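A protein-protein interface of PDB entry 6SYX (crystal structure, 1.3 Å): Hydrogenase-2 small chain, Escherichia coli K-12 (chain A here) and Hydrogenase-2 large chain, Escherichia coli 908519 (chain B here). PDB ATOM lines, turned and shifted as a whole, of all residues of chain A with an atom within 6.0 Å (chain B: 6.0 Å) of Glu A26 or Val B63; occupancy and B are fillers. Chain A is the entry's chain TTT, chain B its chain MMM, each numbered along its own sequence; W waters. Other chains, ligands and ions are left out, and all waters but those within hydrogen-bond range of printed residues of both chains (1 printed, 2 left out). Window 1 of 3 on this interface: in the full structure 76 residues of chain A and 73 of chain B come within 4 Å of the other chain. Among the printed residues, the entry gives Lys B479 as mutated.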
ATOM      1  N   CYS A  21     -19.458 -19.686  19.440  1.00  0.00           N
ATOM      2  CA  CYS A  21     -18.496 -20.683  18.907  1.00  0.00           C
ATOM      3  C   CYS A  21     -18.874 -21.146  17.496  1.00  0.00           C
ATOM      4  O   CYS A  21     -18.105 -21.907  16.855  1.00  0.00           O
ATOM      5  CB  CYS A  21     -18.391 -21.885  19.850  1.00  0.00           C
ATOM      6  SG  CYS A  21     -19.723 -23.127  19.676  1.00  0.00           S
ATOM      7  N   THR A  22     -20.050 -20.740  16.990  1.00  0.00           N
ATOM      8  CA  THR A  22     -20.634 -21.049  15.657  1.00  0.00           C
ATOM      9  C   THR A  22     -21.382 -22.412  15.679  1.00  0.00           C
ATOM     10  O   THR A  22     -22.065 -22.726  14.669  1.00  0.00           O
ATOM     11  CB  THR A  22     -19.630 -20.893  14.496  1.00  0.00           C
ATOM     12  OG1 THR A  22     -19.018 -19.608  14.726  1.00  0.00           O
ATOM     13  CG2 THR A  22     -20.225 -20.896  13.102  1.00  0.00           C
ATOM     14  N   GLY A  23     -21.372 -23.134  16.806  1.00  0.00           N
ATOM     15  CA  GLY A  23     -22.120 -24.386  16.863  1.00  0.00           C
ATOM     16  C   GLY A  23     -23.620 -24.236  16.702  1.00  0.00           C
ATOM     17  O   GLY A  23     -24.286 -25.164  16.178  1.00  0.00           O
ATOM     18  N   CYS A  24     -24.190 -23.089  17.085  1.00  0.00           N
ATOM     19  CA  CYS A  24     -25.645 -22.842  16.932  1.00  0.00           C
ATOM     20  C   CYS A  24     -25.994 -22.641  15.461  1.00  0.00           C
ATOM     21  O   CYS A  24     -27.031 -23.183  14.983  1.00  0.00           O
ATOM     22  CB  CYS A  24     -26.103 -21.675  17.826  1.00  0.00           C
ATOM     23  SG  CYS A  24     -26.149 -22.050  19.603  1.00  0.00           S
ATOM     24  N   THR A  25     -25.188 -21.936  14.663  1.00  0.00           N
ATOM     25  CA  THR A  25     -25.329 -21.914  13.184  1.00  0.00           C
ATOM     26  C   THR A  25     -25.087 -23.314  12.574  1.00  0.00           C
ATOM     27  O   THR A  25     -25.889 -23.782  11.706  1.00  0.00           O
ATOM     28  CB  THR A  25     -24.389 -20.902  12.513  1.00  0.00           C
ATOM     29  OG1 THR A  25     -24.844 -19.568  12.858  1.00  0.00           O
ATOM     30  CG2 THR A  25     -24.353 -21.070  11.021  1.00  0.00           C
ATOM     31  N   GLU A  26     -24.041 -24.023  13.018  1.00  0.00           N
ATOM     32  CA  GLU A  26     -23.748 -25.384  12.474  1.00  0.00           C
ATOM     33  C   GLU A  26     -24.902 -26.368  12.732  1.00  0.00           C
ATOM     34  O   GLU A  26     -25.068 -27.311  11.913  1.00  0.00           O
ATOM     35  CB  GLU A  26     -22.441 -25.876  13.097  1.00  0.00           C
ATOM     36  CG  GLU A  26     -21.202 -25.241  12.462  1.00  0.00           C
ATOM     37  CD  GLU A  26     -20.793 -25.839  11.130  1.00  0.00           C
ATOM     38  OE1 GLU A  26     -21.466 -26.725  10.579  1.00  0.00           O
ATOM     39  OE2 GLU A  26     -19.751 -25.308  10.546  1.00  0.00           O
ATOM     40  N   SER A  27     -25.702 -26.191  13.775  1.00  0.00           N
ATOM     41  CA  SER A  27     -26.879 -27.075  13.991  1.00  0.00           C
ATOM     42  C   SER A  27     -27.779 -27.073  12.757  1.00  0.00           C
ATOM     43  O   SER A  27     -28.360 -28.116  12.372  1.00  0.00           O
ATOM     44  CB  SER A  27     -27.651 -26.736  15.252  1.00  0.00           C
ATOM     45  OG  SER A  27     -28.465 -25.570  15.085  1.00  0.00           O
ATOM     46  N   LEU A  28     -27.872 -25.921  12.059  1.00  0.00           N
ATOM     47  CA  LEU A  28     -28.744 -25.820  10.860  1.00  0.00           C
ATOM     48  C   LEU A  28     -28.305 -26.755   9.732  1.00  0.00           C
ATOM     49  O   LEU A  28     -29.133 -27.201   8.924  1.00  0.00           O
ATOM     50  CB  LEU A  28     -28.809 -24.379  10.332  1.00  0.00           C
ATOM     51  CG  LEU A  28     -29.291 -23.312  11.311  1.00  0.00           C
ATOM     52  CD1 LEU A  28     -29.249 -21.934  10.627  1.00  0.00           C
ATOM     53  CD2 LEU A  28     -30.684 -23.620  11.838  1.00  0.00           C
ATOM     54  N   LEU A  29     -27.010 -27.078   9.673  1.00  0.00           N
ATOM     55  CA  LEU A  29     -26.451 -27.970   8.625  1.00  0.00           C
ATOM     56  C   LEU A  29     -26.781 -29.453   8.890  1.00  0.00           C
ATOM     57  O   LEU A  29     -26.544 -30.261   7.982  1.00  0.00           O
ATOM     58  CB  LEU A  29     -24.936 -27.735   8.453  1.00  0.00           C
ATOM     59  CG  LEU A  29     -24.512 -26.627   7.483  1.00  0.00           C
ATOM     60  CD1 LEU A  29     -24.989 -25.250   7.912  1.00  0.00           C
ATOM     61  CD2 LEU A  29     -23.014 -26.583   7.258  1.00  0.00           C
ATOM     62  N   ARG A  30     -27.335 -29.798  10.041  1.00  0.00           N
ATOM     63  CA  ARG A  30     -27.827 -31.171  10.335  1.00  0.00           C
ATOM     64  C   ARG A  30     -29.350 -31.234  10.145  1.00  0.00           C
ATOM     65  O   ARG A  30     -29.901 -32.376  10.138  1.00  0.00           O
ATOM     66  CB  ARG A  30     -27.485 -31.563  11.783  1.00  0.00           C
ATOM     67  CG  ARG A  30     -26.020 -31.891  12.107  1.00  0.00           C
ATOM     68  CD  ARG A  30     -25.128 -30.672  12.074  1.00  0.00           C
ATOM     69  NE  ARG A  30     -23.819 -30.909  12.686  1.00  0.00           N
ATOM     70  CZ  ARG A  30     -22.712 -30.202  12.460  1.00  0.00           C
ATOM     71  NH1 ARG A  30     -22.738 -29.148  11.638  1.00  0.00           N
ATOM     72  NH2 ARG A  30     -21.581 -30.518  13.093  1.00  0.00           N
ATOM     73  N   GLU B  14     -15.184 -18.768  10.241  1.00  0.00           N
ATOM     74  CA  GLU B  14     -15.706 -18.830  11.623  1.00  0.00           C
ATOM     75  C   GLU B  14     -15.205 -17.590  12.395  1.00  0.00           C
ATOM     76  O   GLU B  14     -13.971 -17.331  12.401  1.00  0.00           O
ATOM     77  CB  GLU B  14     -15.264 -20.129  12.325  1.00  0.00           C
ATOM     78  CG  GLU B  14     -16.026 -20.359  13.625  1.00  0.00           C
ATOM     79  CD  GLU B  14     -15.736 -19.371  14.755  1.00  0.00           C
ATOM     80  OE1 GLU B  14     -14.537 -18.913  14.853  1.00  0.00           O
ATOM     81  OE2 GLU B  14     -16.665 -19.013  15.591  1.00  0.00           O
ATOM     82  N   CYS B  61     -14.834 -24.111  19.910  1.00  0.00           N
ATOM     83  CA  CYS B  61     -15.320 -23.991  18.502  1.00  0.00           C
ATOM     84  C   CYS B  61     -16.354 -25.033  18.142  1.00  0.00           C
ATOM     85  O   CYS B  61     -16.132 -26.248  18.443  1.00  0.00           O
ATOM     86  CB  CYS B  61     -14.139 -24.027  17.541  1.00  0.00           C
ATOM     87  SG  CYS B  61     -14.561 -23.660  15.813  1.00  0.00           S
ATOM     88  N   GLY B  62     -17.402 -24.603  17.442  1.00  0.00           N
ATOM     89  CA  GLY B  62     -18.467 -25.476  16.938  1.00  0.00           C
ATOM     90  C   GLY B  62     -18.322 -25.804  15.475  1.00  0.00           C
ATOM     91  O   GLY B  62     -19.104 -26.706  15.014  1.00  0.00           O
ATOM     92  N   VAL B  63     -17.461 -25.131  14.705  1.00  0.00           N
ATOM     93  CA  VAL B  63     -17.144 -25.526  13.317  1.00  0.00           C
ATOM     94  C   VAL B  63     -16.190 -26.720  13.436  1.00  0.00           C
ATOM     95  O   VAL B  63     -16.571 -27.834  12.996  1.00  0.00           O
ATOM     96  CB  VAL B  63     -16.563 -24.378  12.456  1.00  0.00           C
ATOM     97  CG1 VAL B  63     -16.122 -24.908  11.100  1.00  0.00           C
ATOM     98  CG2 VAL B  63     -17.574 -23.221  12.354  1.00  0.00           C
ATOM     99  N   CYS B  64     -15.043 -26.592  14.114  1.00  0.00           N
ATOM    100  CA  CYS B  64     -14.143 -27.742  14.414  1.00  0.00           C
ATOM    101  C   CYS B  64     -14.563 -28.378  15.735  1.00  0.00           C
ATOM    102  O   CYS B  64     -13.744 -28.623  16.642  1.00  0.00           O
ATOM    103  CB  CYS B  64     -12.671 -27.348  14.343  1.00  0.00           C
ATOM    104  SG  CYS B  64     -12.124 -26.085  15.510  1.00  0.00           S
ATOM    105  N   THR B  65     -15.862 -28.665  15.866  1.00  0.00           N
ATOM    106  CA  THR B  65     -16.358 -29.524  16.978  1.00  0.00           C
ATOM    107  C   THR B  65     -15.612 -30.862  16.917  1.00  0.00           C
ATOM    108  O   THR B  65     -14.977 -31.193  15.877  1.00  0.00           O
ATOM    109  CB  THR B  65     -17.892 -29.595  16.941  1.00  0.00           C
ATOM    110  OG1 THR B  65     -18.299 -30.211  18.157  1.00  0.00           O
ATOM    111  CG2 THR B  65     -18.394 -30.383  15.760  1.00  0.00           C
ATOM    112  N   HIS B  99     -15.867 -36.175  10.837  1.00  0.00           N
ATOM    113  CA  HIS B  99     -16.002 -34.708  11.097  1.00  0.00           C
ATOM    114  C   HIS B  99     -15.186 -33.919  10.063  1.00  0.00           C
ATOM    115  O   HIS B  99     -15.706 -32.951   9.497  1.00  0.00           O
ATOM    116  CB  HIS B  99     -15.570 -34.351  12.532  1.00  0.00           C
ATOM    117  CG  HIS B  99     -15.557 -32.860  12.659  1.00  0.00           C
ATOM    118  ND1 HIS B  99     -16.716 -32.131  12.812  1.00  0.00           N
ATOM    119  CD2 HIS B  99     -14.563 -31.982  12.327  1.00  0.00           C
ATOM    120  CE1 HIS B  99     -16.425 -30.840  12.652  1.00  0.00           C
ATOM    121  NE2 HIS B  99     -15.120 -30.746  12.330  1.00  0.00           N
ATOM    122  N   HIS B 102     -16.852 -33.597   6.615  1.00  0.00           N
ATOM    123  CA  HIS B 102     -17.869 -32.494   6.652  1.00  0.00           C
ATOM    124  C   HIS B 102     -17.138 -31.132   6.575  1.00  0.00           C
ATOM    125  O   HIS B 102     -17.602 -30.242   5.828  1.00  0.00           O
ATOM    126  CB  HIS B 102     -18.761 -32.625   7.905  1.00  0.00           C
ATOM    127  CG  HIS B 102     -19.154 -31.320   8.527  1.00  0.00           C
ATOM    128  ND1 HIS B 102     -20.294 -30.576   8.174  1.00  0.00           N
ATOM    129  CD2 HIS B 102     -18.577 -30.669   9.566  1.00  0.00           C
ATOM    130  CE1 HIS B 102     -20.315 -29.495   8.956  1.00  0.00           C
ATOM    131  NE2 HIS B 102     -19.266 -29.497   9.811  1.00  0.00           N
ATOM    132  N   ASP B 103     -16.106 -30.939   7.372  1.00  0.00           N
ATOM    133  CA  ASP B 103     -15.465 -29.609   7.565  1.00  0.00           C
ATOM    134  C   ASP B 103     -14.851 -29.136   6.233  1.00  0.00           C
ATOM    135  O   ASP B 103     -15.138 -27.991   5.777  1.00  0.00           O
ATOM    136  CB  ASP B 103     -14.435 -29.781   8.698  1.00  0.00           C
ATOM    137  CG  ASP B 103     -13.983 -28.550   9.423  1.00  0.00           C
ATOM    138  OD1 ASP B 103     -13.525 -27.631   8.676  1.00  0.00           O
ATOM    139  OD2 ASP B 103     -13.918 -28.539  10.724  1.00  0.00           O
ATOM    140  N   VAL B 106     -17.637 -28.328   3.431  1.00  0.00           N
ATOM    141  CA  VAL B 106     -18.313 -27.049   3.699  1.00  0.00           C
ATOM    142  C   VAL B 106     -17.352 -25.900   3.418  1.00  0.00           C
ATOM    143  O   VAL B 106     -17.800 -24.823   2.877  1.00  0.00           O
ATOM    144  CB  VAL B 106     -18.881 -27.029   5.122  1.00  0.00           C
ATOM    145  CG1 VAL B 106     -19.405 -25.651   5.591  1.00  0.00           C
ATOM    146  CG2 VAL B 106     -20.005 -28.074   5.246  1.00  0.00           C
ATOM    147  N   LEU B 111     -18.143 -21.782   2.104  1.00  0.00           N
ATOM    148  CA  LEU B 111     -17.296 -20.641   2.558  1.00  0.00           C
ATOM    149  C   LEU B 111     -16.455 -20.042   1.409  1.00  0.00           C
ATOM    150  O   LEU B 111     -16.362 -18.802   1.332  1.00  0.00           O
ATOM    151  CB  LEU B 111     -16.429 -21.043   3.752  1.00  0.00           C
ATOM    152  CG  LEU B 111     -17.205 -21.659   4.930  1.00  0.00           C
ATOM    153  CD1 LEU B 111     -16.299 -21.958   6.113  1.00  0.00           C
ATOM    154  CD2 LEU B 111     -18.378 -20.808   5.353  1.00  0.00           C
ATOM    155  N   GLN B 198     -22.183 -33.597   3.133  1.00  0.00           N
ATOM    156  CA  GLN B 198     -21.721 -33.234   4.496  1.00  0.00           C
ATOM    157  C   GLN B 198     -22.749 -33.731   5.540  1.00  0.00           C
ATOM    158  O   GLN B 198     -22.320 -34.066   6.706  1.00  0.00           O
ATOM    159  CB  GLN B 198     -21.371 -31.743   4.571  1.00  0.00           C
ATOM    160  CG  GLN B 198     -22.562 -30.792   4.479  1.00  0.00           C
ATOM    161  CD  GLN B 198     -23.369 -30.575   5.742  1.00  0.00           C
ATOM    162  OE1 GLN B 198     -22.825 -30.634   6.865  1.00  0.00           O
ATOM    163  NE2 GLN B 198     -24.679 -30.280   5.592  1.00  0.00           N
ATOM    164  N   ASN B 202     -21.875 -36.197   8.896  1.00  0.00           N
ATOM    165  CA  ASN B 202     -22.261 -35.896  10.298  1.00  0.00           C
ATOM    166  C   ASN B 202     -23.206 -36.959  10.911  1.00  0.00           C
ATOM    167  O   ASN B 202     -23.221 -37.083  12.143  1.00  0.00           O
ATOM    168  CB  ASN B 202     -22.764 -34.489  10.463  1.00  0.00           C
ATOM    169  CG  ASN B 202     -21.566 -33.542  10.623  1.00  0.00           C
ATOM    170  OD1 ASN B 202     -21.720 -32.381  10.307  1.00  0.00           O
ATOM    171  ND2 ASN B 202     -20.408 -34.003  11.126  1.00  0.00           N
ATOM    172  N   PRO B 213     -23.625 -30.731  16.357  1.00  0.00           N
ATOM    173  CA  PRO B 213     -22.370 -30.346  17.030  1.00  0.00           C
ATOM    174  C   PRO B 213     -22.235 -30.742  18.506  1.00  0.00           C
ATOM    175  O   PRO B 213     -23.251 -30.916  19.217  1.00  0.00           O
ATOM    176  CB  PRO B 213     -22.341 -28.788  16.888  1.00  0.00           C
ATOM    177  CG  PRO B 213     -23.297 -28.507  15.750  1.00  0.00           C
ATOM    178  CD  PRO B 213     -24.359 -29.536  15.868  1.00  0.00           C
ATOM    179  N   LYS B 479      -7.789 -27.617  10.378  1.00  0.00           N
ATOM    180  CA  LYS B 479      -6.980 -26.400  10.099  1.00  0.00           C
ATOM    181  C   LYS B 479      -5.493 -26.594  10.431  1.00  0.00           C
ATOM    182  O   LYS B 479      -4.705 -25.634  10.148  1.00  0.00           O
ATOM    183  CB  LYS B 479      -7.514 -25.193  10.863  1.00  0.00           C
ATOM    184  CG  LYS B 479      -8.548 -24.324  10.109  1.00  0.00           C
ATOM    185  CD  LYS B 479     -10.035 -24.484  10.530  1.00  0.00           C
ATOM    186  CE  LYS B 479     -10.658 -25.766  10.007  1.00  0.00           C
ATOM    187  NZ  LYS B 479     -12.108 -25.568   9.679  1.00  0.00           N
ATOM    188  N   ASP B 544      -8.597 -21.098   5.652  1.00  0.00           N
ATOM    189  CA  ASP B 544      -9.770 -21.544   6.460  1.00  0.00           C
ATOM    190  C   ASP B 544      -9.753 -20.933   7.853  1.00  0.00           C
ATOM    191  O   ASP B 544      -9.689 -21.633   8.878  1.00  0.00           O
ATOM    192  CB  ASP B 544      -9.742 -23.067   6.505  1.00  0.00           C
ATOM    193  CG  ASP B 544     -10.990 -23.778   6.966  1.00  0.00           C
ATOM    194  OD1 ASP B 544     -12.007 -23.135   7.334  1.00  0.00           O
ATOM    195  OD2 ASP B 544     -10.873 -25.040   7.039  1.00  0.00           O
ATOM    196  N   CYS B 546     -10.391 -19.598  11.530  1.00  0.00           N
ATOM    197  CA  CYS B 546     -11.303 -19.894  12.658  1.00  0.00           C
ATOM    198  C   CYS B 546     -10.864 -19.045  13.835  1.00  0.00           C
ATOM    199  O   CYS B 546      -9.819 -19.367  14.464  1.00  0.00           O
ATOM    200  CB  CYS B 546     -11.303 -21.372  13.016  1.00  0.00           C
ATOM    201  SG  CYS B 546     -12.549 -21.751  14.273  1.00  0.00           S
HETATM  202  O   HOH W   1     -18.595 -26.672   8.686  1.00  0.00           O
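O of Cys A21 lies within hydrogen-bond range of N of Gly B62 (2.8 Å). OG1 of Thr A22 lies within hydrogen-bond range of OE2 of Glu B14 (2.6 Å). The side-chain amide nitrogen of Gln B198 lies within hydrogen-bond range of the backbone carbonyl oxygen of Leu A29 (3.0 Å). The side-chain amide oxygen of Asn B202 sits close to the guanidinium group of Arg A30 (3.4 Å). The backbone carbonyl oxygen of Cys A21 lies close to the side-chain carboxylate of Glu B14.
The backbone NH (N) of Gly A23 lies close to the side-chain sulfur (SG) of Cys A21 (3.3 Å). The side-chain hydroxyl of Ser A27 is in hydrogen-bond range of the backbone carbonyl oxygen of Cys A24, 2.8 Å away. The guanidinium group (NH1) of Arg A30 lies within salt-bridge range of the side-chain carboxylate (OE1) of Glu A26. A ring nitrogen (ND1) of His B102 sits at hydrogen-bond distance from the side-chain amide oxygen (OE1) of Gln B198, at 2.9 Å. OD1 of Asn B202 sits at hydrogen-bond distance from ND1 of His B102, at 3.1 Å. The backbone carbonyl oxygen (O) of Val B106 sits at hydrogen-bond distance from the backbone NH (N) of Leu B111 (3.2 Å).
Among the printed residues, pairs that only touch across the chains: Glu A26 with His B102, Arg A30 with Pro B213, Gly A23 with Pro B213, Glu A26 with Val B63, Thr A22 with Val B63, Glu A26 with Gly B62, Arg A30 with His B102, Gly A23 with Gly B62, Cys A21 with Cys B61, Glu A26 with Pro B213, Ser A27 with Pro B213, Leu A29 with Val B106 and Cys A21 with Val B63.
Of the printed residues of chain B, Cys A21 touches Glu B14, Cys B61, Gly B62 and Val B63. Printed residues of chain B within 4 Å of Thr A22: Glu B14 (2.6 Å) and Val B63 (3.6 Å). Glu A26 touches just these residues of chain B: Gly B62 (3.6 Å), Val B63 (3.5 Å), His B102 (3.4 Å) and Pro B213 (3.8 Å). Printed residues of chain B within 4 Å of Leu A29: Val B106 and Gln B198. Of the printed residues of chain A, Val B63 touches Cys A21, Thr A22 and Glu A26. The nearest residue of chain A that does not touch Val B63 is Gly A23 (4.9 Å).
Hydrophobic or aromatic side chains of chain B within 4 Å of the printed part of chain A: Val B63, His B102, Val B106 and Pro B213. Along chain B the printed residues that touch a printed residue of chain A span positions 14 to 213. Among the printed residues, 18 pairs touch across the chains. Among the printed residues, no Asp or Glu carboxylate lies within 4 Å of a Lys or Arg side-chain nitrogen of the other chain.
Water W1 lies within hydrogen-bond range of OE2 of Glu A26 (2.6 Å) and NE2 of His B102 (3.1 Å).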
